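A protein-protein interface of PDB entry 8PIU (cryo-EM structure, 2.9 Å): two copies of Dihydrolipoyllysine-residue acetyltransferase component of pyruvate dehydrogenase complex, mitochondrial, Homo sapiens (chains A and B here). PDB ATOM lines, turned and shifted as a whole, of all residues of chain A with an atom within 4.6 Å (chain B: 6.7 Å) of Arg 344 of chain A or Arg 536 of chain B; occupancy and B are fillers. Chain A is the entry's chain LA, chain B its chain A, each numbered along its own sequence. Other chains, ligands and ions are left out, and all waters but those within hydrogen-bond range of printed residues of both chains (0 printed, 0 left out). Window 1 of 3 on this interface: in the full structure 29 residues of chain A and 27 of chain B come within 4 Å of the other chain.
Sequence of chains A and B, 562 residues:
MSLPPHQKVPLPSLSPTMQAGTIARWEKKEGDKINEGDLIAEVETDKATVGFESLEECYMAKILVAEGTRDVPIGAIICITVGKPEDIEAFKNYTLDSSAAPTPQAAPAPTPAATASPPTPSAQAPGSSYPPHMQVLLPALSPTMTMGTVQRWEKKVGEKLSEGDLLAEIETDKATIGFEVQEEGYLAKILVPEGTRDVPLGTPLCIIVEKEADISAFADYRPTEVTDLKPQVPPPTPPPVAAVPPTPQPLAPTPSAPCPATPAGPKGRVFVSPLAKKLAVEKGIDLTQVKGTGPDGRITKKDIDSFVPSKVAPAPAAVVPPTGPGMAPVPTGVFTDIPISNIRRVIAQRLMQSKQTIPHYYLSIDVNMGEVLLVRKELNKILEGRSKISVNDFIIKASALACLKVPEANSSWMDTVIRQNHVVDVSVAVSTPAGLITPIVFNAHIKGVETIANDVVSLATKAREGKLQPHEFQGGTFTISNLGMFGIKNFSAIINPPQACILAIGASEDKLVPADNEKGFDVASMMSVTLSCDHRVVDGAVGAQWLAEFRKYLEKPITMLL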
ATOM      1  N   ILE A 340       8.138  16.996   7.666  1.00  0.00           N
ATOM      2  CA  ILE A 340       8.747  18.305   7.870  1.00  0.00           C
ATOM      3  C   ILE A 340       8.625  19.113   6.587  1.00  0.00           C
ATOM      4  O   ILE A 340       8.990  18.636   5.505  1.00  0.00           O
ATOM      5  CB  ILE A 340      10.219  18.172   8.297  1.00  0.00           C
ATOM      6  CG1 ILE A 340      10.347  17.181   9.453  1.00  0.00           C
ATOM      7  CG2 ILE A 340      10.779  19.525   8.696  1.00  0.00           C
ATOM      8  CD1 ILE A 340      11.772  16.911   9.868  1.00  0.00           C
ATOM      9  N   SER A 341       8.112  20.334   6.706  1.00  0.00           N
ATOM     10  CA  SER A 341       7.997  21.220   5.560  1.00  0.00           C
ATOM     11  C   SER A 341       9.369  21.750   5.151  1.00  0.00           C
ATOM     12  O   SER A 341      10.344  21.675   5.902  1.00  0.00           O
ATOM     13  CB  SER A 341       7.056  22.383   5.874  1.00  0.00           C
ATOM     14  OG  SER A 341       7.517  23.121   6.993  1.00  0.00           O
ATOM     15  N   ASN A 342       9.435  22.291   3.933  1.00  0.00           N
ATOM     16  CA  ASN A 342      10.698  22.822   3.425  1.00  0.00           C
ATOM     17  C   ASN A 342      11.143  24.049   4.210  1.00  0.00           C
ATOM     18  O   ASN A 342      12.343  24.243   4.440  1.00  0.00           O
ATOM     19  CB  ASN A 342      10.570  23.148   1.939  1.00  0.00           C
ATOM     20  CG  ASN A 342      10.292  21.920   1.097  1.00  0.00           C
ATOM     21  OD1 ASN A 342      11.215  21.244   0.640  1.00  0.00           O
ATOM     22  ND2 ASN A 342       9.015  21.622   0.887  1.00  0.00           N
ATOM     23  N   ILE A 343      10.196  24.897   4.617  1.00  0.00           N
ATOM     24  CA  ILE A 343      10.541  26.072   5.414  1.00  0.00           C
ATOM     25  C   ILE A 343      11.150  25.647   6.743  1.00  0.00           C
ATOM     26  O   ILE A 343      12.187  26.169   7.172  1.00  0.00           O
ATOM     27  CB  ILE A 343       9.304  26.968   5.620  1.00  0.00           C
ATOM     28  CG1 ILE A 343       8.941  27.705   4.325  1.00  0.00           C
ATOM     29  CG2 ILE A 343       9.542  27.959   6.749  1.00  0.00           C
ATOM     30  CD1 ILE A 343       8.051  26.917   3.384  1.00  0.00           C
ATOM     31  N   ARG A 344      10.518  24.680   7.411  1.00  0.00           N
ATOM     32  CA  ARG A 344      11.069  24.171   8.661  1.00  0.00           C
ATOM     33  C   ARG A 344      12.427  23.523   8.436  1.00  0.00           C
ATOM     34  O   ARG A 344      13.334  23.671   9.260  1.00  0.00           O
ATOM     35  CB  ARG A 344      10.101  23.178   9.303  1.00  0.00           C
ATOM     36  CG  ARG A 344       8.891  23.819   9.955  1.00  0.00           C
ATOM     37  CD  ARG A 344       8.096  22.790  10.740  1.00  0.00           C
ATOM     38  NE  ARG A 344       8.948  22.041  11.655  1.00  0.00           N
ATOM     39  CZ  ARG A 344       9.235  22.423  12.892  1.00  0.00           C
ATOM     40  NH1 ARG A 344       8.745  23.540  13.402  1.00  0.00           N
ATOM     41  NH2 ARG A 344      10.036  21.665  13.635  1.00  0.00           N
ATOM     42  N   ARG A 345      12.587  22.804   7.323  1.00  0.00           N
ATOM     43  CA  ARG A 345      13.861  22.155   7.033  1.00  0.00           C
ATOM     44  C   ARG A 345      14.980  23.176   6.874  1.00  0.00           C
ATOM     45  O   ARG A 345      16.066  23.019   7.446  1.00  0.00           O
ATOM     46  CB  ARG A 345      13.733  21.295   5.775  1.00  0.00           C
ATOM     47  CG  ARG A 345      15.060  20.806   5.222  1.00  0.00           C
ATOM     48  CD  ARG A 345      15.752  19.860   6.188  1.00  0.00           C
ATOM     49  NE  ARG A 345      15.050  18.587   6.301  1.00  0.00           N
ATOM     50  CZ  ARG A 345      15.302  17.525   5.549  1.00  0.00           C
ATOM     51  NH1 ARG A 345      16.239  17.547   4.615  1.00  0.00           N
ATOM     52  NH2 ARG A 345      14.599  16.413   5.739  1.00  0.00           N
ATOM     53  N   VAL A 346      14.735  24.236   6.101  1.00  0.00           N
ATOM     54  CA  VAL A 346      15.783  25.228   5.873  1.00  0.00           C
ATOM     55  C   VAL A 346      16.065  26.016   7.148  1.00  0.00           C
ATOM     56  O   VAL A 346      17.219  26.352   7.440  1.00  0.00           O
ATOM     57  CB  VAL A 346      15.428  26.145   4.685  1.00  0.00           C
ATOM     58  CG1 VAL A 346      15.283  25.326   3.411  1.00  0.00           C
ATOM     59  CG2 VAL A 346      14.170  26.950   4.954  1.00  0.00           C
ATOM     60  N   ILE A 347      15.027  26.314   7.938  1.00  0.00           N
ATOM     61  CA  ILE A 347      15.245  27.002   9.208  1.00  0.00           C
ATOM     62  C   ILE A 347      16.080  26.138  10.147  1.00  0.00           C
ATOM     63  O   ILE A 347      17.001  26.627  10.813  1.00  0.00           O
ATOM     64  CB  ILE A 347      13.900  27.397   9.844  1.00  0.00           C
ATOM     65  CG1 ILE A 347      13.234  28.509   9.033  1.00  0.00           C
ATOM     66  CG2 ILE A 347      14.094  27.834  11.287  1.00  0.00           C
ATOM     67  CD1 ILE A 347      11.888  28.936   9.575  1.00  0.00           C
ATOM     68  N   ALA A 348      15.772  24.840  10.212  1.00  0.00           N
ATOM     69  CA  ALA A 348      16.538  23.932  11.056  1.00  0.00           C
ATOM     70  C   ALA A 348      17.983  23.833  10.591  1.00  0.00           C
ATOM     71  O   ALA A 348      18.905  23.808  11.415  1.00  0.00           O
ATOM     72  CB  ALA A 348      15.885  22.550  11.067  1.00  0.00           C
ATOM     73  N   SER B 354      25.495  14.425  20.389  1.00  0.00           N
ATOM     74  CA  SER B 354      24.308  15.181  20.774  1.00  0.00           C
ATOM     75  C   SER B 354      24.593  16.676  20.798  1.00  0.00           C
ATOM     76  O   SER B 354      23.825  17.476  20.250  1.00  0.00           O
ATOM     77  CB  SER B 354      23.809  14.714  22.140  1.00  0.00           C
ATOM     78  OG  SER B 354      22.814  15.591  22.641  1.00  0.00           O
ATOM     79  N   THR B 357      24.978  17.961  17.162  1.00  0.00           N
ATOM     80  CA  THR B 357      23.837  17.932  16.256  1.00  0.00           C
ATOM     81  C   THR B 357      22.636  18.722  16.758  1.00  0.00           C
ATOM     82  O   THR B 357      21.914  19.305  15.943  1.00  0.00           O
ATOM     83  CB  THR B 357      23.413  16.484  15.992  1.00  0.00           C
ATOM     84  OG1 THR B 357      23.178  15.817  17.238  1.00  0.00           O
ATOM     85  CG2 THR B 357      24.495  15.746  15.220  1.00  0.00           C
ATOM     86  N   ILE B 358      22.397  18.762  18.062  1.00  0.00           N
ATOM     87  CA  ILE B 358      21.202  19.383  18.624  1.00  0.00           C
ATOM     88  C   ILE B 358      21.541  20.821  19.004  1.00  0.00           C
ATOM     89  O   ILE B 358      22.426  21.031  19.846  1.00  0.00           O
ATOM     90  CB  ILE B 358      20.680  18.605  19.839  1.00  0.00           C
ATOM     91  CG1 ILE B 358      20.316  17.175  19.435  1.00  0.00           C
ATOM     92  CG2 ILE B 358      19.486  19.313  20.447  1.00  0.00           C
ATOM     93  CD1 ILE B 358      19.792  16.333  20.573  1.00  0.00           C
ATOM     94  N   PRO B 359      20.886  21.824  18.417  1.00  0.00           N
ATOM     95  CA  PRO B 359      21.055  23.208  18.876  1.00  0.00           C
ATOM     96  C   PRO B 359      20.258  23.461  20.147  1.00  0.00           C
ATOM     97  O   PRO B 359      19.035  23.628  20.112  1.00  0.00           O
ATOM     98  CB  PRO B 359      20.524  24.030  17.694  1.00  0.00           C
ATOM     99  CG  PRO B 359      19.551  23.130  17.023  1.00  0.00           C
ATOM    100  CD  PRO B 359      20.099  21.744  17.174  1.00  0.00           C
ATOM    101  N   TYR B 361      18.818  25.382  23.455  1.00  0.00           N
ATOM    102  CA  TYR B 361      18.554  26.706  24.000  1.00  0.00           C
ATOM    103  C   TYR B 361      17.803  26.545  25.312  1.00  0.00           C
ATOM    104  O   TYR B 361      16.962  25.658  25.448  1.00  0.00           O
ATOM    105  CB  TYR B 361      17.786  27.595  23.014  1.00  0.00           C
ATOM    106  CG  TYR B 361      16.320  27.296  22.897  1.00  0.00           C
ATOM    107  CD1 TYR B 361      15.864  26.310  22.041  1.00  0.00           C
ATOM    108  CD2 TYR B 361      15.386  28.014  23.628  1.00  0.00           C
ATOM    109  CE1 TYR B 361      14.523  26.036  21.925  1.00  0.00           C
ATOM    110  CE2 TYR B 361      14.044  27.745  23.521  1.00  0.00           C
ATOM    111  CZ  TYR B 361      13.619  26.753  22.668  1.00  0.00           C
ATOM    112  OH  TYR B 361      12.281  26.477  22.554  1.00  0.00           O
ATOM    113  N   TRP B 413      13.149  14.399  16.835  1.00  0.00           N
ATOM    114  CA  TRP B 413      13.608  14.760  15.499  1.00  0.00           C
ATOM    115  C   TRP B 413      14.299  13.561  14.868  1.00  0.00           C
ATOM    116  O   TRP B 413      15.198  12.968  15.474  1.00  0.00           O
ATOM    117  CB  TRP B 413      14.561  15.956  15.553  1.00  0.00           C
ATOM    118  CG  TRP B 413      15.172  16.316  14.231  1.00  0.00           C
ATOM    119  CD1 TRP B 413      16.286  15.767  13.666  1.00  0.00           C
ATOM    120  CD2 TRP B 413      14.711  17.315  13.315  1.00  0.00           C
ATOM    121  NE1 TRP B 413      16.543  16.356  12.453  1.00  0.00           N
ATOM    122  CE2 TRP B 413      15.589  17.310  12.215  1.00  0.00           C
ATOM    123  CE3 TRP B 413      13.639  18.210  13.317  1.00  0.00           C
ATOM    124  CZ2 TRP B 413      15.429  18.165  11.129  1.00  0.00           C
ATOM    125  CZ3 TRP B 413      13.482  19.057  12.239  1.00  0.00           C
ATOM    126  CH2 TRP B 413      14.372  19.029  11.160  1.00  0.00           C
ATOM    127  N   ASP B 415      15.306  13.702  11.337  1.00  0.00           N
ATOM    128  CA  ASP B 415      15.822  14.197  10.064  1.00  0.00           C
ATOM    129  C   ASP B 415      14.737  14.244   8.997  1.00  0.00           C
ATOM    130  O   ASP B 415      14.294  15.325   8.599  1.00  0.00           O
ATOM    131  CB  ASP B 415      16.999  13.340   9.588  1.00  0.00           C
ATOM    132  CG  ASP B 415      18.122  13.282  10.602  1.00  0.00           C
ATOM    133  OD1 ASP B 415      18.291  14.263  11.357  1.00  0.00           O
ATOM    134  OD2 ASP B 415      18.833  12.257  10.648  1.00  0.00           O
ATOM    135  N   ILE B 418       9.378  14.127  11.860  1.00  0.00           N
ATOM    136  CA  ILE B 418       9.304  14.466  13.277  1.00  0.00           C
ATOM    137  C   ILE B 418       8.306  13.520  13.927  1.00  0.00           C
ATOM    138  O   ILE B 418       7.131  13.487  13.545  1.00  0.00           O
ATOM    139  CB  ILE B 418       8.899  15.930  13.496  1.00  0.00           C
ATOM    140  CG1 ILE B 418      10.060  16.864  13.152  1.00  0.00           C
ATOM    141  CG2 ILE B 418       8.443  16.150  14.929  1.00  0.00           C
ATOM    142  CD1 ILE B 418       9.781  18.317  13.456  1.00  0.00           C
ATOM    143  N   PRO B 497      20.403  12.431  22.365  1.00  0.00           N
ATOM    144  CA  PRO B 497      20.317  12.608  20.904  1.00  0.00           C
ATOM    145  C   PRO B 497      18.927  12.349  20.340  1.00  0.00           C
ATOM    146  O   PRO B 497      18.487  13.094  19.452  1.00  0.00           O
ATOM    147  CB  PRO B 497      21.337  11.592  20.371  1.00  0.00           C
ATOM    148  CG  PRO B 497      22.338  11.486  21.462  1.00  0.00           C
ATOM    149  CD  PRO B 497      21.573  11.625  22.752  1.00  0.00           C
ATOM    150  N   CYS B 533      15.778  23.029  25.464  1.00  0.00           N
ATOM    151  CA  CYS B 533      14.979  22.593  24.334  1.00  0.00           C
ATOM    152  C   CYS B 533      15.810  22.551  23.055  1.00  0.00           C
ATOM    153  O   CYS B 533      16.826  23.239  22.908  1.00  0.00           O
ATOM    154  CB  CYS B 533      13.777  23.512  24.143  1.00  0.00           C
ATOM    155  SG  CYS B 533      12.977  24.022  25.666  1.00  0.00           S
ATOM    156  N   ASP B 534      15.349  21.723  22.123  1.00  0.00           N
ATOM    157  CA  ASP B 534      15.898  21.620  20.778  1.00  0.00           C
ATOM    158  C   ASP B 534      15.126  22.598  19.901  1.00  0.00           C
ATOM    159  O   ASP B 534      13.920  22.435  19.697  1.00  0.00           O
ATOM    160  CB  ASP B 534      15.776  20.191  20.257  1.00  0.00           C
ATOM    161  CG  ASP B 534      16.415  20.008  18.904  1.00  0.00           C
ATOM    162  OD1 ASP B 534      17.129  20.927  18.458  1.00  0.00           O
ATOM    163  OD2 ASP B 534      16.206  18.945  18.285  1.00  0.00           O
ATOM    164  N   HIS B 535      15.823  23.613  19.385  1.00  0.00           N
ATOM    165  CA  HIS B 535      15.136  24.720  18.730  1.00  0.00           C
ATOM    166  C   HIS B 535      14.572  24.343  17.368  1.00  0.00           C
ATOM    167  O   HIS B 535      13.678  25.036  16.871  1.00  0.00           O
ATOM    168  CB  HIS B 535      16.077  25.913  18.594  1.00  0.00           C
ATOM    169  CG  HIS B 535      15.371  27.232  18.534  1.00  0.00           C
ATOM    170  ND1 HIS B 535      16.041  28.430  18.421  1.00  0.00           N
ATOM    171  CD2 HIS B 535      14.054  27.540  18.576  1.00  0.00           C
ATOM    172  CE1 HIS B 535      15.167  29.420  18.394  1.00  0.00           C
ATOM    173  NE2 HIS B 535      13.954  28.908  18.487  1.00  0.00           N
ATOM    174  N   ARG B 536      15.065  23.274  16.751  1.00  0.00           N
ATOM    175  CA  ARG B 536      14.496  22.822  15.491  1.00  0.00           C
ATOM    176  C   ARG B 536      13.227  22.006  15.685  1.00  0.00           C
ATOM    177  O   ARG B 536      12.585  21.642  14.694  1.00  0.00           O
ATOM    178  CB  ARG B 536      15.530  22.010  14.707  1.00  0.00           C
ATOM    179  CG  ARG B 536      16.097  20.845  15.475  1.00  0.00           C
ATOM    180  CD  ARG B 536      17.208  20.157  14.713  1.00  0.00           C
ATOM    181  NE  ARG B 536      17.736  19.025  15.464  1.00  0.00           N
ATOM    182  CZ  ARG B 536      18.615  18.156  14.990  1.00  0.00           C
ATOM    183  NH1 ARG B 536      19.095  18.259  13.763  1.00  0.00           N
ATOM    184  NH2 ARG B 536      19.020  17.156  15.766  1.00  0.00           N
ATOM    185  N   VAL B 537      12.855  21.713  16.930  1.00  0.00           N
ATOM    186  CA  VAL B 537      11.621  21.011  17.256  1.00  0.00           C
ATOM    187  C   VAL B 537      10.724  21.853  18.156  1.00  0.00           C
ATOM    188  O   VAL B 537       9.511  21.931  17.946  1.00  0.00           O
ATOM    189  CB  VAL B 537      11.908  19.638  17.903  1.00  0.00           C
ATOM    190  CG1 VAL B 537      10.614  18.932  18.253  1.00  0.00           C
ATOM    191  CG2 VAL B 537      12.744  18.783  16.974  1.00  0.00           C
ATOM    192  N   VAL B 538      11.308  22.499  19.162  1.00  0.00           N
ATOM    193  CA  VAL B 538      10.564  23.279  20.143  1.00  0.00           C
ATOM    194  C   VAL B 538      10.888  24.752  19.938  1.00  0.00           C
ATOM    195  O   VAL B 538      12.061  25.145  19.950  1.00  0.00           O
ATOM    196  CB  VAL B 538      10.893  22.843  21.578  1.00  0.00           C
ATOM    197  CG1 VAL B 538      10.015  23.582  22.571  1.00  0.00           C
ATOM    198  CG2 VAL B 538      10.732  21.344  21.727  1.00  0.00           C
ATOM    199  N   ASP B 539       9.853  25.565  19.751  1.00  0.00           N
ATOM    200  CA  ASP B 539      10.020  27.006  19.679  1.00  0.00           C
ATOM    201  C   ASP B 539      10.061  27.604  21.083  1.00  0.00           C
ATOM    202  O   ASP B 539       9.715  26.958  22.076  1.00  0.00           O
ATOM    203  CB  ASP B 539       8.893  27.640  18.867  1.00  0.00           C
ATOM    204  CG  ASP B 539       8.799  27.077  17.464  1.00  0.00           C
ATOM    205  OD1 ASP B 539       9.567  26.144  17.145  1.00  0.00           O
ATOM    206  OD2 ASP B 539       7.958  27.566  16.681  1.00  0.00           O
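Among the printed residues, pairs that only touch across the chains: Ile 340 of chain A with Trp 413 of chain B, Ile 340 of chain A with Asp 415 of chain B, Ile 340 of chain A with Ile 418 of chain B, Arg 344 of chain A with Ile 418 of chain B, Ala 348 of chain A with Trp 413 of chain B and Ala 348 of chain A with Arg 536 of chain B.
Of the 9 printed residues of chain A, 4 touch a printed residue of chain B.
Hydrophobic or aromatic side chains of chain B within 4 Å of the printed part of chain A: Trp 413 and Ile 418.
Among the printed residues, 8 pairs touch across the chains.
Among the printed residues, no Asp or Glu carboxylate lies within 4 Å of a Lys or Arg side-chain nitrogen of the other chain.
The indole nitrogen (NE1) of Trp 413 of chain B sits at hydrogen-bond distance from the side-chain carboxylate (OD1) of Asp 415 of chain B, at 2.9 Å.
The side-chain carboxylate (OD2) of Asp 534 of chain B lies within salt-bridge range of the guanidinium group (NE) of Arg 536 of chain B (3.2 Å).
The side-chain hydroxyl (OG) of Ser 341 of chain A lies close to the backbone NH (N) of Arg 344 of chain A.
The guanidinium group (NH2) of Arg 345 of chain A lies within hydrogen-bond range of the backbone carbonyl oxygen (O) of Asp 415 of chain B (3.1 Å).
NH2 of Arg 344 of chain A is in hydrogen-bond range of O of Arg 536 of chain B, at 2.8 Å.
No position is printed for both chains.
Of the 8 pairs that touch across the chains among the printed residues, none has its exchanged pair printed and touching as well.
Of the printed residues of chain B, Arg 344 of chain A touches Ile 418 (3.4 Å) and Arg 536 (2.8 Å).
Arg 536 of chain B touches two residues of chain A.
Printed residues of chain B within 4 Å of Ile 340 of chain A: Trp 413 (3.6 Å), Asp 415 (3.2 Å) and Ile 418 (3.7 Å).
Of the printed residues of chain A, Trp 413 of chain B touches Ile 340 and Ala 348.
Of the printed residues of chain A, Asp 415 of chain B touches Ile 340 (3.2 Å) and Arg 345 (3.1 Å).
Of the printed residues of chain B, Ala 348 of chain A touches Trp 413 and Arg 536.
Val 537 of chain B touches none of the printed residues of chain A.
The nearest printed residue of chain B that does not touch Arg 344 of chain A is Val 537 of chain B (4.01 Å).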
